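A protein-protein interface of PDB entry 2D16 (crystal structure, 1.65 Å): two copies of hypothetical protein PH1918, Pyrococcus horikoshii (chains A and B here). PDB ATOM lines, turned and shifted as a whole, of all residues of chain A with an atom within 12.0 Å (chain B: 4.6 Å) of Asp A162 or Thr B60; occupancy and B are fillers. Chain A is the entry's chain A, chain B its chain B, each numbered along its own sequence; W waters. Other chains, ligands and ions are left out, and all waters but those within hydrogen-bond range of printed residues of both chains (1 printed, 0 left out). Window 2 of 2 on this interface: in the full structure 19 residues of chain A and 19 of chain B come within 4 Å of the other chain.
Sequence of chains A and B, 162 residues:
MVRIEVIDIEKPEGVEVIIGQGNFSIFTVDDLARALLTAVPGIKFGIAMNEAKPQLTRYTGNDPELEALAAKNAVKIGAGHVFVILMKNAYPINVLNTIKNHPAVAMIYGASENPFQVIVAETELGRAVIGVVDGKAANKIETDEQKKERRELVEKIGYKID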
ATOM      1  N   VAL A 154      17.819  24.847  -6.645  1.00  0.00           N
ATOM      2  CA  VAL A 154      18.272  26.092  -7.257  1.00  0.00           C
ATOM      3  C   VAL A 154      19.414  25.817  -8.235  1.00  0.00           C
ATOM      4  O   VAL A 154      19.476  26.407  -9.315  1.00  0.00           O
ATOM      5  CB  VAL A 154      18.733  27.112  -6.191  1.00  0.00           C
ATOM      6  CG1 VAL A 154      19.464  28.274  -6.858  1.00  0.00           C
ATOM      7  CG2 VAL A 154      17.520  27.631  -5.426  1.00  0.00           C
ATOM      8  N   GLU A 155      20.316  24.915  -7.865  1.00  0.00           N
ATOM      9  CA  GLU A 155      21.417  24.591  -8.755  1.00  0.00           C
ATOM     10  C   GLU A 155      20.892  23.830  -9.970  1.00  0.00           C
ATOM     11  O   GLU A 155      21.333  24.068 -11.091  1.00  0.00           O
ATOM     12  CB  GLU A 155      22.483  23.768  -8.027  1.00  0.00           C
ATOM     13  CG  GLU A 155      23.258  24.571  -6.989  1.00  0.00           C
ATOM     14  CD  GLU A 155      24.481  23.838  -6.464  1.00  0.00           C
ATOM     15  OE1 GLU A 155      25.179  24.395  -5.588  1.00  0.00           O
ATOM     16  OE2 GLU A 155      24.748  22.711  -6.927  1.00  0.00           O
ATOM     17  N   LYS A 156      19.934  22.931  -9.749  1.00  0.00           N
ATOM     18  CA  LYS A 156      19.365  22.153 -10.846  1.00  0.00           C
ATOM     19  C   LYS A 156      18.647  23.047 -11.853  1.00  0.00           C
ATOM     20  O   LYS A 156      18.618  22.753 -13.050  1.00  0.00           O
ATOM     21  CB  LYS A 156      18.388  21.099 -10.310  1.00  0.00           C
ATOM     22  CG  LYS A 156      17.755  20.247 -11.408  1.00  0.00           C
ATOM     23  CD  LYS A 156      16.789  19.211 -10.848  1.00  0.00           C
ATOM     24  CE  LYS A 156      16.146  18.405 -11.974  1.00  0.00           C
ATOM     25  NZ  LYS A 156      15.208  17.361 -11.469  1.00  0.00           N
ATOM     26  N   GLY A 158      19.575  25.891 -12.806  1.00  0.00           N
ATOM     27  CA  GLY A 158      20.556  26.519 -13.673  1.00  0.00           C
ATOM     28  C   GLY A 158      21.439  27.539 -12.982  1.00  0.00           C
ATOM     29  O   GLY A 158      22.362  28.085 -13.593  1.00  0.00           O
ATOM     30  N   TYR A 159      21.160  27.811 -11.713  1.00  0.00           N
ATOM     31  CA  TYR A 159      21.961  28.770 -10.966  1.00  0.00           C
ATOM     32  C   TYR A 159      23.139  28.022 -10.364  1.00  0.00           C
ATOM     33  O   TYR A 159      23.188  27.738  -9.168  1.00  0.00           O
ATOM     34  CB  TYR A 159      21.097  29.442  -9.898  1.00  0.00           C
ATOM     35  CG  TYR A 159      20.022  30.305 -10.520  1.00  0.00           C
ATOM     36  CD1 TYR A 159      20.326  31.563 -11.049  1.00  0.00           C
ATOM     37  CD2 TYR A 159      18.716  29.842 -10.637  1.00  0.00           C
ATOM     38  CE1 TYR A 159      19.349  32.334 -11.684  1.00  0.00           C
ATOM     39  CE2 TYR A 159      17.731  30.602 -11.271  1.00  0.00           C
ATOM     40  CZ  TYR A 159      18.055  31.846 -11.791  1.00  0.00           C
ATOM     41  OH  TYR A 159      17.083  32.592 -12.422  1.00  0.00           O
ATOM     42  N   LYS A 160      24.085  27.703 -11.239  1.00  0.00           N
ATOM     43  CA  LYS A 160      25.282  26.960 -10.880  1.00  0.00           C
ATOM     44  C   LYS A 160      26.433  27.441 -11.757  1.00  0.00           C
ATOM     45  O   LYS A 160      26.254  27.668 -12.954  1.00  0.00           O
ATOM     46  CB  LYS A 160      25.040  25.466 -11.126  1.00  0.00           C
ATOM     47  CG  LYS A 160      26.205  24.557 -10.782  1.00  0.00           C
ATOM     48  CD  LYS A 160      26.455  24.515  -9.284  1.00  0.00           C
ATOM     49  CE  LYS A 160      27.490  23.451  -8.940  1.00  0.00           C
ATOM     50  NZ  LYS A 160      27.049  22.098  -9.393  1.00  0.00           N
ATOM     51  N   ILE A 161      27.607  27.595 -11.159  1.00  0.00           N
ATOM     52  CA  ILE A 161      28.786  28.035 -11.895  1.00  0.00           C
ATOM     53  C   ILE A 161      29.906  27.021 -11.694  1.00  0.00           C
ATOM     54  O   ILE A 161      29.923  26.292 -10.701  1.00  0.00           O
ATOM     55  CB  ILE A 161      29.273  29.425 -11.421  1.00  0.00           C
ATOM     56  CG1 ILE A 161      29.702  29.363  -9.955  1.00  0.00           C
ATOM     57  CG2 ILE A 161      28.169  30.448 -11.615  1.00  0.00           C
ATOM     58  CD1 ILE A 161      30.321  30.649  -9.437  1.00  0.00           C
ATOM     59  N   ASP A 162      30.837  26.980 -12.641  1.00  0.00           N
ATOM     60  CA  ASP A 162      31.958  26.048 -12.583  1.00  0.00           C
ATOM     61  C   ASP A 162      33.050  26.497 -11.617  1.00  0.00           C
ATOM     62  O   ASP A 162      33.519  27.649 -11.729  1.00  0.00           O
ATOM     63  CB  ASP A 162      32.532  25.867 -13.989  1.00  0.00           C
ATOM     64  CG  ASP A 162      31.529  25.258 -14.949  1.00  0.00           C
ATOM     65  OD1 ASP A 162      31.711  25.393 -16.178  1.00  0.00           O
ATOM     66  OD2 ASP A 162      30.555  24.633 -14.473  1.00  0.00           O
ATOM     67  OXT ASP A 162      33.438  25.682 -10.753  1.00  0.00           O
ATOM     68  N   VAL B  29      34.726  37.457  -9.253  1.00  0.00           N
ATOM     69  CA  VAL B  29      34.666  36.573 -10.406  1.00  0.00           C
ATOM     70  C   VAL B  29      33.472  35.622 -10.273  1.00  0.00           C
ATOM     71  O   VAL B  29      32.744  35.393 -11.238  1.00  0.00           O
ATOM     72  CB  VAL B  29      35.986  35.778 -10.588  1.00  0.00           C
ATOM     73  CG1 VAL B  29      36.151  34.757  -9.482  1.00  0.00           C
ATOM     74  CG2 VAL B  29      36.004  35.117 -11.962  1.00  0.00           C
ATOM     75  N   ASP B  30      33.259  35.093  -9.072  1.00  0.00           N
ATOM     76  CA  ASP B  30      32.141  34.186  -8.816  1.00  0.00           C
ATOM     77  C   ASP B  30      30.814  34.925  -8.645  1.00  0.00           C
ATOM     78  O   ASP B  30      29.786  34.507  -9.173  1.00  0.00           O
ATOM     79  CB  ASP B  30      32.378  33.374  -7.539  1.00  0.00           C
ATOM     80  CG  ASP B  30      33.306  32.195  -7.748  1.00  0.00           C
ATOM     81  OD1 ASP B  30      33.731  31.955  -8.895  1.00  0.00           O
ATOM     82  OD2 ASP B  30      33.600  31.503  -6.749  1.00  0.00           O
ATOM     83  N   ALA B  33      29.409  36.358 -11.851  1.00  0.00           N
ATOM     84  CA  ALA B  33      28.945  35.251 -12.686  1.00  0.00           C
ATOM     85  C   ALA B  33      27.527  34.884 -12.238  1.00  0.00           C
ATOM     86  O   ALA B  33      26.637  34.684 -13.062  1.00  0.00           O
ATOM     87  CB  ALA B  33      29.881  34.043 -12.539  1.00  0.00           C
ATOM     88  N   PHE B  45      28.042  31.610 -20.638  1.00  0.00           N
ATOM     89  CA  PHE B  45      29.175  32.516 -20.594  1.00  0.00           C
ATOM     90  C   PHE B  45      30.385  32.033 -19.823  1.00  0.00           C
ATOM     91  O   PHE B  45      30.355  31.026 -19.105  1.00  0.00           O
ATOM     92  CB  PHE B  45      28.722  33.823 -19.951  1.00  0.00           C
ATOM     93  CG  PHE B  45      28.420  33.686 -18.483  1.00  0.00           C
ATOM     94  CD1 PHE B  45      29.402  33.947 -17.530  1.00  0.00           C
ATOM     95  CD2 PHE B  45      27.171  33.233 -18.052  1.00  0.00           C
ATOM     96  CE1 PHE B  45      29.150  33.755 -16.168  1.00  0.00           C
ATOM     97  CE2 PHE B  45      26.907  33.037 -16.690  1.00  0.00           C
ATOM     98  CZ  PHE B  45      27.899  33.298 -15.749  1.00  0.00           C
ATOM     99  N   GLY B  46      31.449  32.805 -19.985  1.00  0.00           N
ATOM    100  CA  GLY B  46      32.685  32.567 -19.282  1.00  0.00           C
ATOM    101  C   GLY B  46      33.084  33.941 -18.780  1.00  0.00           C
ATOM    102  O   GLY B  46      32.853  34.938 -19.467  1.00  0.00           O
ATOM    103  N   ILE B  47      33.632  34.012 -17.574  1.00  0.00           N
ATOM    104  CA  ILE B  47      34.088  35.282 -17.030  1.00  0.00           C
ATOM    105  C   ILE B  47      35.429  35.048 -16.350  1.00  0.00           C
ATOM    106  O   ILE B  47      35.612  34.060 -15.637  1.00  0.00           O
ATOM    107  CB  ILE B  47      33.080  35.888 -16.009  1.00  0.00           C
ATOM    108  CG1 ILE B  47      33.601  37.246 -15.517  1.00  0.00           C
ATOM    109  CG2 ILE B  47      32.869  34.936 -14.831  1.00  0.00           C
ATOM    110  CD1 ILE B  47      32.608  38.003 -14.643  1.00  0.00           C
ATOM    111  N   TYR B  59      38.794  32.588 -13.036  1.00  0.00           N
ATOM    112  CA  TYR B  59      37.707  32.438 -13.991  1.00  0.00           C
ATOM    113  C   TYR B  59      36.641  31.430 -13.581  1.00  0.00           C
ATOM    114  O   TYR B  59      36.866  30.560 -12.737  1.00  0.00           O
ATOM    115  CB  TYR B  59      38.272  32.063 -15.369  1.00  0.00           C
ATOM    116  CG  TYR B  59      38.708  30.617 -15.496  1.00  0.00           C
ATOM    117  CD1 TYR B  59      37.823  29.640 -15.958  1.00  0.00           C
ATOM    118  CD2 TYR B  59      39.995  30.220 -15.135  1.00  0.00           C
ATOM    119  CE1 TYR B  59      38.210  28.300 -16.056  1.00  0.00           C
ATOM    120  CE2 TYR B  59      40.393  28.882 -15.228  1.00  0.00           C
ATOM    121  CZ  TYR B  59      39.494  27.931 -15.689  1.00  0.00           C
ATOM    122  OH  TYR B  59      39.874  26.608 -15.777  1.00  0.00           O
ATOM    123  N   THR B  60      35.470  31.572 -14.187  1.00  0.00           N
ATOM    124  CA  THR B  60      34.345  30.682 -13.940  1.00  0.00           C
ATOM    125  C   THR B  60      33.295  30.938 -15.013  1.00  0.00           C
ATOM    126  O   THR B  60      33.563  31.639 -15.990  1.00  0.00           O
ATOM    127  CB  THR B  60      33.731  30.899 -12.534  1.00  0.00           C
ATOM    128  OG1 THR B  60      32.660  29.965 -12.330  1.00  0.00           O
ATOM    129  CG2 THR B  60      33.199  32.321 -12.387  1.00  0.00           C
ATOM    130  N   GLY B  61      32.111  30.365 -14.833  1.00  0.00           N
ATOM    131  CA  GLY B  61      31.044  30.532 -15.799  1.00  0.00           C
ATOM    132  C   GLY B  61      30.258  29.242 -15.907  1.00  0.00           C
ATOM    133  O   GLY B  61      30.281  28.422 -14.988  1.00  0.00           O
ATOM    134  N   ASN B  62      29.564  29.053 -17.025  1.00  0.00           N
ATOM    135  CA  ASN B  62      28.780  27.840 -17.228  1.00  0.00           C
ATOM    136  C   ASN B  62      28.963  27.286 -18.638  1.00  0.00           C
ATOM    137  O   ASN B  62      28.073  26.625 -19.177  1.00  0.00           O
ATOM    138  CB  ASN B  62      27.294  28.110 -16.953  1.00  0.00           C
ATOM    139  CG  ASN B  62      26.681  29.085 -17.938  1.00  0.00           C
ATOM    140  OD1 ASN B  62      27.371  29.656 -18.780  1.00  0.00           O
ATOM    141  ND2 ASN B  62      25.372  29.283 -17.833  1.00  0.00           N
ATOM    142  N   ASP B  63      30.122  27.567 -19.226  1.00  0.00           N
ATOM    143  CA  ASP B  63      30.460  27.100 -20.571  1.00  0.00           C
ATOM    144  C   ASP B  63      31.976  26.910 -20.639  1.00  0.00           C
ATOM    145  O   ASP B  63      32.736  27.879 -20.599  1.00  0.00           O
ATOM    146  CB  ASP B  63      30.025  28.121 -21.626  1.00  0.00           C
ATOM    147  CG  ASP B  63      30.140  27.578 -23.041  1.00  0.00           C
ATOM    148  OD1 ASP B  63      29.189  26.909 -23.502  1.00  0.00           O
ATOM    149  OD2 ASP B  63      31.183  27.803 -23.687  1.00  0.00           O
ATOM    150  N   GLU B  67      34.752  29.940 -21.062  1.00  0.00           N
ATOM    151  CA  GLU B  67      35.538  30.164 -19.858  1.00  0.00           C
ATOM    152  C   GLU B  67      37.020  30.161 -20.218  1.00  0.00           C
ATOM    153  O   GLU B  67      37.776  31.038 -19.797  1.00  0.00           O
ATOM    154  CB  GLU B  67      35.247  29.074 -18.828  1.00  0.00           C
ATOM    155  CG  GLU B  67      33.882  29.211 -18.168  1.00  0.00           C
ATOM    156  CD  GLU B  67      33.541  28.035 -17.283  1.00  0.00           C
ATOM    157  OE1 GLU B  67      34.442  27.550 -16.565  1.00  0.00           O
ATOM    158  OE2 GLU B  67      32.369  27.603 -17.294  1.00  0.00           O
HETATM  159  O   HOH W   1      24.156  27.589 -15.496  1.00  0.00           O
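Water W1 lies within hydrogen-bond range of O of Gly A158, ND2 of Asn B62 and O of Lys A160.
No position is printed for both chains.
Of the 7 pairs that touch across the chains among the printed residues, none has its exchanged pair printed and touching as well.
Ile A161 touches Asp B30 (CD1 to OD1, 3.7 Å).
Thr B60 touches Ile A161 (OG1 to CB, 3.5 Å).
O of Gly B61 touches CA of Ile A161 (3.5 Å).
CA of Asn B62 touches OD1 of Asp A162, 3.96 Å away.
Gly A158 touches none of the printed residues of chain B.
Printed residues of chain B within 4 Å of Ile A161: Asp B30, Thr B60 and Gly B61.
Of chain B, only Thr B60 (2.5 Å), Gly B61 (2.8 Å), Asn B62 (3.96 Å) and Glu B67 (2.6 Å) come within 4 Å of Asp A162.
Val B29 touches none of the printed residues of chain A.
Printed residues of chain A within 4 Å of Asp B30: Ile A161 (3.7 Å).
No residue of chain A comes within 4 Å of Ala B33.
No residue of chain A comes within 4 Å of Phe B45.
No residue of chain A comes within 4 Å of Ile B47.
No residue of chain A comes within 4 Å of Tyr B59.
Thr B60 touches just these residues of chain A: Ile A161 (3.5 Å) and Asp A162 (2.5 Å).
Asn B62 touches one residue of chain A.
Glu B67 touches just one residue of chain A: Asp A162.
The nearest residue of chain A that does not touch Thr B60 is Lys A160 (6.7 Å).
The side-chain hydroxyl (OG1) of Thr B60 is in hydrogen-bond range of the chain-end carboxylate (O) of Asp A162 (2.5 Å).
O of Gly B61 sits at hydrogen-bond distance from N of Asp A162 (2.8 Å).
The side-chain carboxylate (OD1) of Asp A162 sits close to the side-chain carboxylate (OE2) of Glu B67 (2.6 Å).
Of the 8 printed residues of chain A, 2 touch a printed residue of chain B.
Hydrophobic or aromatic side chains of chain A within 4 Å of the printed part of chain B: Ile A161.
Among the printed residues, no Asp or Glu carboxylate lies within 4 Å of a Lys or Arg side-chain nitrogen of the other chain.
The backbone NH of Ile B47 is in hydrogen-bond range of the backbone carbonyl oxygen of Thr B60, at 2.9 Å.
The side-chain carboxylate (OE2) of Glu B67 lies within hydrogen-bond range of the backbone NH (N) of Asn B62 (3.2 Å).
OD1 of Asn B62 sits at hydrogen-bond distance from N of Phe B45 (2.8 Å).
The side-chain carboxylate of Glu B67 is in hydrogen-bond range of the backbone NH of Asp B63 (3.0 Å).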
